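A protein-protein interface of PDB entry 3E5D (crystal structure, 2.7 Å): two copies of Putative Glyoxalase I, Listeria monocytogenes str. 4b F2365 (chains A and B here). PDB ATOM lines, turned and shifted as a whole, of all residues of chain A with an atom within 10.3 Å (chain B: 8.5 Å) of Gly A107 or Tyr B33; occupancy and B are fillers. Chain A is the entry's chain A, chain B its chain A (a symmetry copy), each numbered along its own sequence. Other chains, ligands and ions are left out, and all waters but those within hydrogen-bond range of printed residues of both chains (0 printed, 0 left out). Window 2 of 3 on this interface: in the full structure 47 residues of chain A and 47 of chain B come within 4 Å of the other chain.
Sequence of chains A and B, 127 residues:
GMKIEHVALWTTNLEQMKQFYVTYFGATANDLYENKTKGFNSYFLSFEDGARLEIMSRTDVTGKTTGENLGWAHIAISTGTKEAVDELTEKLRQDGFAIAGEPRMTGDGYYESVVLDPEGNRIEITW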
ATOM      1  N   ARG A 104       8.959  30.993  11.835  1.00  0.00           N
ATOM      2  CA  ARG A 104      10.310  30.671  11.413  1.00  0.00           C
ATOM      3  C   ARG A 104      10.409  30.512   9.895  1.00  0.00           C
ATOM      4  O   ARG A 104       9.390  30.404   9.206  1.00  0.00           O
ATOM      5  CB  ARG A 104      10.754  29.370  12.072  1.00  0.00           C
ATOM      6  CG  ARG A 104      10.164  28.129  11.449  1.00  0.00           C
ATOM      7  CD  ARG A 104      10.596  26.884  12.215  1.00  0.00           C
ATOM      8  NE  ARG A 104      10.995  25.800  11.315  1.00  0.00           N
ATOM      9  CZ  ARG A 104      10.159  25.041  10.607  1.00  0.00           C
ATOM     10  NH1 ARG A 104       8.840  25.235  10.654  1.00  0.00           N
ATOM     11  NH2 ARG A 104      10.651  24.092   9.821  1.00  0.00           N
ATOM     12  N   MET A 105      11.640  30.514   9.393  1.00  0.00           N
ATOM     13  CA  MET A 105      11.916  30.224   7.991  1.00  0.00           C
ATOM     14  C   MET A 105      11.956  28.722   7.846  1.00  0.00           C
ATOM     15  O   MET A 105      12.756  28.066   8.501  1.00  0.00           O
ATOM     16  CB  MET A 105      13.262  30.798   7.525  1.00  0.00           C
ATOM     17  CG  MET A 105      13.140  32.098   6.763  1.00  0.00           C
ATOM     18  SD  MET A 105      12.303  31.758   5.057  1.00  0.00           S
ATOM     19  CE  MET A 105      13.733  30.502   4.346  1.00  0.00           C
ATOM     20  N   THR A 106      11.101  28.178   6.992  1.00  0.00           N
ATOM     21  CA  THR A 106      11.069  26.745   6.789  1.00  0.00           C
ATOM     22  C   THR A 106      12.115  26.405   5.736  1.00  0.00           C
ATOM     23  O   THR A 106      12.603  27.291   5.031  1.00  0.00           O
ATOM     24  CB  THR A 106       9.695  26.291   6.327  1.00  0.00           C
ATOM     25  OG1 THR A 106       9.425  26.876   5.051  1.00  0.00           O
ATOM     26  CG2 THR A 106       8.626  26.731   7.326  1.00  0.00           C
ATOM     27  N   GLY A 107      12.458  25.125   5.632  1.00  0.00           N
ATOM     28  CA  GLY A 107      13.445  24.671   4.660  1.00  0.00           C
ATOM     29  C   GLY A 107      13.004  24.827   3.213  1.00  0.00           C
ATOM     30  O   GLY A 107      13.836  24.846   2.316  1.00  0.00           O
ATOM     31  N   ASP A 108      11.695  24.911   2.988  1.00  0.00           N
ATOM     32  CA  ASP A 108      11.141  25.074   1.640  1.00  0.00           C
ATOM     33  C   ASP A 108      10.888  26.545   1.351  1.00  0.00           C
ATOM     34  O   ASP A 108      10.172  26.862   0.411  1.00  0.00           O
ATOM     35  CB  ASP A 108       9.868  24.211   1.400  1.00  0.00           C
ATOM     36  CG  ASP A 108       8.816  24.321   2.534  1.00  0.00           C
ATOM     37  OD1 ASP A 108       9.029  25.063   3.520  1.00  0.00           O
ATOM     38  OD2 ASP A 108       7.776  23.621   2.464  1.00  0.00           O
ATOM     39  N   GLY A 109      11.441  27.434   2.185  1.00  0.00           N
ATOM     40  CA  GLY A 109      11.388  28.896   1.958  1.00  0.00           C
ATOM     41  C   GLY A 109      10.190  29.748   2.360  1.00  0.00           C
ATOM     42  O   GLY A 109       9.898  30.736   1.699  1.00  0.00           O
ATOM     43  N   TYR A 110       9.519  29.397   3.451  1.00  0.00           N
ATOM     44  CA  TYR A 110       8.360  30.148   3.929  1.00  0.00           C
ATOM     45  C   TYR A 110       8.647  30.686   5.300  1.00  0.00           C
ATOM     46  O   TYR A 110       9.278  30.003   6.112  1.00  0.00           O
ATOM     47  CB  TYR A 110       7.106  29.249   3.999  1.00  0.00           C
ATOM     48  CG  TYR A 110       6.648  28.887   2.632  1.00  0.00           C
ATOM     49  CD1 TYR A 110       7.403  28.020   1.871  1.00  0.00           C
ATOM     50  CD2 TYR A 110       5.499  29.453   2.062  1.00  0.00           C
ATOM     51  CE1 TYR A 110       7.054  27.703   0.579  1.00  0.00           C
ATOM     52  CE2 TYR A 110       5.118  29.129   0.748  1.00  0.00           C
ATOM     53  CZ  TYR A 110       5.926  28.249   0.020  1.00  0.00           C
ATOM     54  OH  TYR A 110       5.668  27.846  -1.264  1.00  0.00           O
ATOM     55  N   TYR A 111       8.237  31.923   5.551  1.00  0.00           N
ATOM     56  CA  TYR A 111       8.284  32.432   6.898  1.00  0.00           C
ATOM     57  C   TYR A 111       6.862  32.210   7.386  1.00  0.00           C
ATOM     58  O   TYR A 111       5.913  32.848   6.893  1.00  0.00           O
ATOM     59  CB  TYR A 111       8.667  33.897   7.000  1.00  0.00           C
ATOM     60  CG  TYR A 111       8.838  34.279   8.451  1.00  0.00           C
ATOM     61  CD1 TYR A 111      10.030  34.014   9.117  1.00  0.00           C
ATOM     62  CD2 TYR A 111       7.795  34.850   9.177  1.00  0.00           C
ATOM     63  CE1 TYR A 111      10.196  34.335  10.453  1.00  0.00           C
ATOM     64  CE2 TYR A 111       7.955  35.173  10.532  1.00  0.00           C
ATOM     65  CZ  TYR A 111       9.161  34.913  11.161  1.00  0.00           C
ATOM     66  OH  TYR A 111       9.342  35.225  12.495  1.00  0.00           O
ATOM     67  N   GLU A 112       6.695  31.299   8.334  1.00  0.00           N
ATOM     68  CA  GLU A 112       5.360  30.986   8.787  1.00  0.00           C
ATOM     69  C   GLU A 112       5.310  30.462  10.192  1.00  0.00           C
ATOM     70  O   GLU A 112       6.327  30.071  10.753  1.00  0.00           O
ATOM     71  CB  GLU A 112       4.765  29.918   7.870  1.00  0.00           C
ATOM     72  CG  GLU A 112       5.560  28.605   7.863  1.00  0.00           C
ATOM     73  CD  GLU A 112       4.835  27.482   7.134  1.00  0.00           C
ATOM     74  OE1 GLU A 112       4.132  27.781   6.141  1.00  0.00           O
ATOM     75  OE2 GLU A 112       4.973  26.308   7.558  1.00  0.00           O
ATOM     76  N   GLU A 124      -1.373  27.375   8.387  1.00  0.00           N
ATOM     77  CA  GLU A 124      -0.027  27.934   8.327  1.00  0.00           C
ATOM     78  C   GLU A 124      -0.232  29.413   8.120  1.00  0.00           C
ATOM     79  O   GLU A 124      -0.946  29.796   7.209  1.00  0.00           O
ATOM     80  CB  GLU A 124       0.789  27.369   7.159  1.00  0.00           C
ATOM     81  CG  GLU A 124       1.241  25.932   7.337  1.00  0.00           C
ATOM     82  CD  GLU A 124       2.073  25.385   6.165  1.00  0.00           C
ATOM     83  OE1 GLU A 124       2.177  26.041   5.111  1.00  0.00           O
ATOM     84  OE2 GLU A 124       2.626  24.270   6.299  1.00  0.00           O
ATOM     85  N   LEU B  14       3.277  10.424  -4.593  1.00  0.00           N
ATOM     86  CA  LEU B  14       3.477  11.821  -5.021  1.00  0.00           C
ATOM     87  C   LEU B  14       3.475  12.080  -6.521  1.00  0.00           C
ATOM     88  O   LEU B  14       2.802  12.996  -6.974  1.00  0.00           O
ATOM     89  CB  LEU B  14       4.744  12.418  -4.376  1.00  0.00           C
ATOM     90  CG  LEU B  14       4.953  13.945  -4.412  1.00  0.00           C
ATOM     91  CD1 LEU B  14       3.876  14.689  -3.621  1.00  0.00           C
ATOM     92  CD2 LEU B  14       6.332  14.315  -3.879  1.00  0.00           C
ATOM     93  N   GLU B  15       4.196  11.282  -7.298  1.00  0.00           N
ATOM     94  CA  GLU B  15       4.269  11.525  -8.746  1.00  0.00           C
ATOM     95  C   GLU B  15       2.943  11.284  -9.457  1.00  0.00           C
ATOM     96  O   GLU B  15       2.560  12.052 -10.341  1.00  0.00           O
ATOM     97  CB  GLU B  15       5.372  10.678  -9.393  1.00  0.00           C
ATOM     98  CG  GLU B  15       6.786  11.026  -8.928  1.00  0.00           C
ATOM     99  CD  GLU B  15       7.205  12.467  -9.253  1.00  0.00           C
ATOM    100  OE1 GLU B  15       6.656  13.082 -10.197  1.00  0.00           O
ATOM    101  OE2 GLU B  15       8.096  12.989  -8.562  1.00  0.00           O
ATOM    102  N   ASN B  30       6.287  22.887  -9.622  1.00  0.00           N
ATOM    103  CA  ASN B  30       7.573  23.521  -9.399  1.00  0.00           C
ATOM    104  C   ASN B  30       8.568  22.372  -9.261  1.00  0.00           C
ATOM    105  O   ASN B  30       8.266  21.235  -9.635  1.00  0.00           O
ATOM    106  CB  ASN B  30       7.543  24.386  -8.140  1.00  0.00           C
ATOM    107  CG  ASN B  30       7.378  23.576  -6.860  1.00  0.00           C
ATOM    108  OD1 ASN B  30       6.940  22.425  -6.871  1.00  0.00           O
ATOM    109  ND2 ASN B  30       7.716  24.190  -5.746  1.00  0.00           N
ATOM    110  N   ASP B  31       9.746  22.650  -8.715  1.00  0.00           N
ATOM    111  CA  ASP B  31      10.745  21.608  -8.521  1.00  0.00           C
ATOM    112  C   ASP B  31      10.434  20.828  -7.260  1.00  0.00           C
ATOM    113  O   ASP B  31       9.940  21.383  -6.283  1.00  0.00           O
ATOM    114  CB  ASP B  31      12.148  22.204  -8.418  1.00  0.00           C
ATOM    115  CG  ASP B  31      12.653  22.772  -9.741  1.00  0.00           C
ATOM    116  OD1 ASP B  31      12.140  22.379 -10.816  1.00  0.00           O
ATOM    117  OD2 ASP B  31      13.591  23.597  -9.700  1.00  0.00           O
ATOM    118  N   LEU B  32      10.708  19.531  -7.306  1.00  0.00           N
ATOM    119  CA  LEU B  32      10.516  18.667  -6.166  1.00  0.00           C
ATOM    120  C   LEU B  32      11.321  19.220  -4.994  1.00  0.00           C
ATOM    121  O   LEU B  32      12.465  19.600  -5.168  1.00  0.00           O
ATOM    122  CB  LEU B  32      11.014  17.256  -6.507  1.00  0.00           C
ATOM    123  CG  LEU B  32      10.946  16.187  -5.409  1.00  0.00           C
ATOM    124  CD1 LEU B  32       9.490  15.923  -5.010  1.00  0.00           C
ATOM    125  CD2 LEU B  32      11.634  14.906  -5.865  1.00  0.00           C
ATOM    126  N   TYR B  33      10.701  19.335  -3.824  1.00  0.00           N
ATOM    127  CA  TYR B  33      11.423  19.716  -2.614  1.00  0.00           C
ATOM    128  C   TYR B  33      11.619  18.430  -1.848  1.00  0.00           C
ATOM    129  O   TYR B  33      10.765  17.539  -1.877  1.00  0.00           O
ATOM    130  CB  TYR B  33      10.665  20.726  -1.748  1.00  0.00           C
ATOM    131  CG  TYR B  33      11.266  20.921  -0.349  1.00  0.00           C
ATOM    132  CD1 TYR B  33      12.445  21.646  -0.151  1.00  0.00           C
ATOM    133  CD2 TYR B  33      10.648  20.376   0.777  1.00  0.00           C
ATOM    134  CE1 TYR B  33      12.989  21.820   1.132  1.00  0.00           C
ATOM    135  CE2 TYR B  33      11.192  20.545   2.062  1.00  0.00           C
ATOM    136  CZ  TYR B  33      12.356  21.265   2.226  1.00  0.00           C
ATOM    137  OH  TYR B  33      12.865  21.418   3.490  1.00  0.00           O
ATOM    138  N   GLU B  34      12.729  18.340  -1.131  1.00  0.00           N
ATOM    139  CA  GLU B  34      13.037  17.119  -0.434  1.00  0.00           C
ATOM    140  C   GLU B  34      13.743  17.388   0.877  1.00  0.00           C
ATOM    141  O   GLU B  34      14.591  18.276   0.959  1.00  0.00           O
ATOM    142  CB  GLU B  34      13.915  16.277  -1.357  1.00  0.00           C
ATOM    143  CG  GLU B  34      13.935  14.799  -1.056  1.00  0.00           C
ATOM    144  CD  GLU B  34      14.574  13.987  -2.180  1.00  0.00           C
ATOM    145  OE1 GLU B  34      15.382  14.563  -2.946  1.00  0.00           O
ATOM    146  OE2 GLU B  34      14.263  12.778  -2.289  1.00  0.00           O
ATOM    147  N   ASN B  35      13.339  16.654   1.911  1.00  0.00           N
ATOM    148  CA  ASN B  35      14.017  16.678   3.209  1.00  0.00           C
ATOM    149  C   ASN B  35      14.288  15.215   3.552  1.00  0.00           C
ATOM    150  O   ASN B  35      13.478  14.550   4.205  1.00  0.00           O
ATOM    151  CB  ASN B  35      13.184  17.381   4.285  1.00  0.00           C
ATOM    152  CG  ASN B  35      13.918  17.498   5.622  1.00  0.00           C
ATOM    153  OD1 ASN B  35      15.036  17.007   5.804  1.00  0.00           O
ATOM    154  ND2 ASN B  35      13.277  18.153   6.563  1.00  0.00           N
ATOM    155  N   LYS B  36      15.421  14.714   3.060  1.00  0.00           N
ATOM    156  CA  LYS B  36      15.790  13.316   3.257  1.00  0.00           C
ATOM    157  C   LYS B  36      15.698  12.905   4.743  1.00  0.00           C
ATOM    158  O   LYS B  36      15.188  11.827   5.040  1.00  0.00           O
ATOM    159  CB  LYS B  36      17.171  13.000   2.629  1.00  0.00           C
ATOM    160  CG  LYS B  36      17.206  12.999   1.076  1.00  0.00           C
ATOM    161  N   LYS B  38      13.667  13.779   7.225  1.00  0.00           N
ATOM    162  CA  LYS B  38      12.302  13.544   7.705  1.00  0.00           C
ATOM    163  C   LYS B  38      11.481  12.668   6.744  1.00  0.00           C
ATOM    164  O   LYS B  38      10.303  12.398   7.003  1.00  0.00           O
ATOM    165  CB  LYS B  38      11.587  14.892   7.906  1.00  0.00           C
ATOM    166  CG  LYS B  38      12.394  15.954   8.697  1.00  0.00           C
ATOM    167  CD  LYS B  38      12.408  15.779  10.234  1.00  0.00           C
ATOM    168  CE  LYS B  38      11.102  16.292  10.868  1.00  0.00           C
ATOM    169  NZ  LYS B  38      11.216  16.404  12.351  1.00  0.00           N
ATOM    170  N   GLY B  39      12.099  12.230   5.645  1.00  0.00           N
ATOM    171  CA  GLY B  39      11.420  11.413   4.625  1.00  0.00           C
ATOM    172  C   GLY B  39      10.301  12.167   3.920  1.00  0.00           C
ATOM    173  O   GLY B  39       9.342  11.572   3.466  1.00  0.00           O
ATOM    174  N   PHE B  40      10.451  13.480   3.796  1.00  0.00           N
ATOM    175  CA  PHE B  40       9.424  14.346   3.229  1.00  0.00           C
ATOM    176  C   PHE B  40       9.706  14.789   1.781  1.00  0.00           C
ATOM    177  O   PHE B  40      10.842  15.113   1.427  1.00  0.00           O
ATOM    178  CB  PHE B  40       9.284  15.572   4.162  1.00  0.00           C
ATOM    179  CG  PHE B  40       8.286  16.598   3.696  1.00  0.00           C
ATOM    180  CD1 PHE B  40       8.666  17.621   2.855  1.00  0.00           C
ATOM    181  CD2 PHE B  40       6.963  16.528   4.091  1.00  0.00           C
ATOM    182  CE1 PHE B  40       7.746  18.557   2.428  1.00  0.00           C
ATOM    183  CE2 PHE B  40       6.052  17.461   3.669  1.00  0.00           C
ATOM    184  CZ  PHE B  40       6.441  18.472   2.835  1.00  0.00           C
ATOM    185  N   ASN B  41       8.667  14.783   0.950  1.00  0.00           N
ATOM    186  CA  ASN B  41       8.754  15.271  -0.434  1.00  0.00           C
ATOM    187  C   ASN B  41       7.540  16.115  -0.762  1.00  0.00           C
ATOM    188  O   ASN B  41       6.462  15.845  -0.245  1.00  0.00           O
ATOM    189  CB  ASN B  41       8.809  14.137  -1.448  1.00  0.00           C
ATOM    190  CG  ASN B  41      10.065  13.337  -1.349  1.00  0.00           C
ATOM    191  OD1 ASN B  41      11.003  13.533  -2.123  1.00  0.00           O
ATOM    192  ND2 ASN B  41      10.113  12.445  -0.378  1.00  0.00           N
ATOM    193  N   SER B  42       7.702  17.124  -1.618  1.00  0.00           N
ATOM    194  CA  SER B  42       6.567  17.955  -2.013  1.00  0.00           C
ATOM    195  C   SER B  42       6.741  18.683  -3.328  1.00  0.00           C
ATOM    196  O   SER B  42       7.851  18.949  -3.785  1.00  0.00           O
ATOM    197  CB  SER B  42       6.272  19.018  -0.951  1.00  0.00           C
ATOM    198  OG  SER B  42       7.263  20.034  -0.932  1.00  0.00           O
ATOM    199  N   TYR B  43       5.595  19.012  -3.908  1.00  0.00           N
ATOM    200  CA  TYR B  43       5.502  19.832  -5.100  1.00  0.00           C
ATOM    201  C   TYR B  43       4.450  20.891  -4.820  1.00  0.00           C
ATOM    202  O   TYR B  43       3.542  20.676  -4.010  1.00  0.00           O
ATOM    203  CB  TYR B  43       5.018  19.039  -6.308  1.00  0.00           C
ATOM    204  CG  TYR B  43       6.000  18.083  -6.958  1.00  0.00           C
ATOM    205  CD1 TYR B  43       7.026  18.553  -7.775  1.00  0.00           C
ATOM    206  CD2 TYR B  43       5.843  16.705  -6.835  1.00  0.00           C
ATOM    207  CE1 TYR B  43       7.898  17.678  -8.400  1.00  0.00           C
ATOM    208  CE2 TYR B  43       6.708  15.827  -7.456  1.00  0.00           C
ATOM    209  CZ  TYR B  43       7.727  16.319  -8.236  1.00  0.00           C
ATOM    210  OH  TYR B  43       8.576  15.441  -8.848  1.00  0.00           O
ATOM    211  N   PHE B  44       4.590  22.033  -5.480  1.00  0.00           N
ATOM    212  CA  PHE B  44       3.575  23.068  -5.459  1.00  0.00           C
ATOM    213  C   PHE B  44       3.033  23.143  -6.873  1.00  0.00           C
ATOM    214  O   PHE B  44       3.796  23.267  -7.842  1.00  0.00           O
ATOM    215  CB  PHE B  44       4.130  24.413  -5.028  1.00  0.00           C
ATOM    216  CG  PHE B  44       4.188  24.587  -3.546  1.00  0.00           C
ATOM    217  CD1 PHE B  44       5.273  24.137  -2.824  1.00  0.00           C
ATOM    218  CD2 PHE B  44       3.142  25.201  -2.873  1.00  0.00           C
ATOM    219  CE1 PHE B  44       5.323  24.299  -1.458  1.00  0.00           C
ATOM    220  CE2 PHE B  44       3.179  25.365  -1.497  1.00  0.00           C
ATOM    221  CZ  PHE B  44       4.275  24.917  -0.791  1.00  0.00           C
ATOM    222  N   GLU B  54      -0.445  22.266  -2.630  1.00  0.00           N
ATOM    223  CA  GLU B  54       0.812  21.675  -2.167  1.00  0.00           C
ATOM    224  C   GLU B  54       0.559  20.210  -1.968  1.00  0.00           C
ATOM    225  O   GLU B  54      -0.214  19.829  -1.081  1.00  0.00           O
ATOM    226  CB  GLU B  54       1.299  22.290  -0.841  1.00  0.00           C
ATOM    227  CG  GLU B  54       2.605  21.668  -0.325  1.00  0.00           C
ATOM    228  CD  GLU B  54       3.188  22.336   0.929  1.00  0.00           C
ATOM    229  OE1 GLU B  54       2.493  23.123   1.631  1.00  0.00           O
ATOM    230  OE2 GLU B  54       4.375  22.052   1.208  1.00  0.00           O
ATOM    231  N   ILE B  55       1.164  19.385  -2.817  1.00  0.00           N
ATOM    232  CA  ILE B  55       1.029  17.929  -2.664  1.00  0.00           C
ATOM    233  C   ILE B  55       2.305  17.442  -2.005  1.00  0.00           C
ATOM    234  O   ILE B  55       3.413  17.764  -2.449  1.00  0.00           O
ATOM    235  CB  ILE B  55       0.723  17.162  -3.971  1.00  0.00           C
ATOM    236  CG1 ILE B  55       1.731  17.495  -5.077  1.00  0.00           C
ATOM    237  CG2 ILE B  55      -0.678  17.477  -4.429  1.00  0.00           C
ATOM    238  CD1 ILE B  55       1.552  16.652  -6.334  1.00  0.00           C
ATOM    239  N   MET B  56       2.148  16.674  -0.936  1.00  0.00           N
ATOM    240  CA  MET B  56       3.291  16.226  -0.178  1.00  0.00           C
ATOM    241  C   MET B  56       3.132  14.807   0.347  1.00  0.00           C
ATOM    242  O   MET B  56       2.040  14.260   0.363  1.00  0.00           O
ATOM    243  CB  MET B  56       3.552  17.231   0.945  1.00  0.00           C
ATOM    244  CG  MET B  56       2.351  17.530   1.827  1.00  0.00           C
ATOM    245  SD  MET B  56       2.527  19.198   2.871  1.00  0.00           S
ATOM    246  CE  MET B  56       1.043  18.743   4.188  1.00  0.00           C
ATOM    247  N   SER B  57       4.250  14.207   0.725  1.00  0.00           N
ATOM    248  CA  SER B  57       4.259  12.871   1.271  1.00  0.00           C
ATOM    249  C   SER B  57       5.412  12.732   2.235  1.00  0.00           C
ATOM    250  O   SER B  57       6.412  13.432   2.108  1.00  0.00           O
ATOM    251  CB  SER B  57       4.457  11.842   0.155  1.00  0.00           C
ATOM    252  OG  SER B  57       5.786  11.871  -0.347  1.00  0.00           O
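The side-chain hydroxyl of Thr A106 sits at hydrogen-bond distance from the side-chain carboxylate of Asp A108, at 2.4 Å.
N of Tyr A110 lies within hydrogen-bond range of OG1 of Thr A106 (3.0 Å).
The backbone NH of Phe B44 is in hydrogen-bond range of the side-chain amide oxygen of Asn B30 (2.8 Å).
The backbone NH (N) of Tyr B33 is in hydrogen-bond range of the backbone carbonyl oxygen (O) of Ser B42 (2.9 Å).
Among the printed residues, pairs that only touch across the chains: Tyr A110 with Phe B44 (3.3 Å), Gly A107 with Tyr B33 (3.4 Å), Asp A108 with Tyr B33 (3.7 Å) and Asp A108 with Glu B54 (3.95 Å).
Gly A107 touches just one residue of chain B: Tyr B33 (3.4 Å).
Printed residues of chain B within 4 Å of Asp A108: Tyr B33 (3.7 Å) and Glu B54 (3.95 Å).
Printed residues of chain B within 4 Å of Tyr A110: Phe B44.
Leu B32 touches none of the printed residues of chain A.
Tyr B33 touches two residues of chain A.
No residue of chain A comes within 4 Å of Asn B41.
Printed residues of chain A within 4 Å of Phe B44: Tyr A110.
Printed residues of chain A within 4 Å of Glu B54: Asp A108.
The nearest printed residue of chain B that does not touch Tyr A110 is Asn B30 (6.1 Å).
Hydrophobic or aromatic side chains of chain A that line the printed part of chain B: Tyr A110.
Of the 20 printed residues of chain B, 3 touch a printed residue of chain A.
Hydrophobic or aromatic side chains of chain B within 4 Å of the printed part of chain A: Tyr B33 and Phe B44.
Among the printed residues, no Asp or Glu carboxylate lies within 4 Å of a Lys or Arg side-chain nitrogen of the other chain.
No position is printed for both chains.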
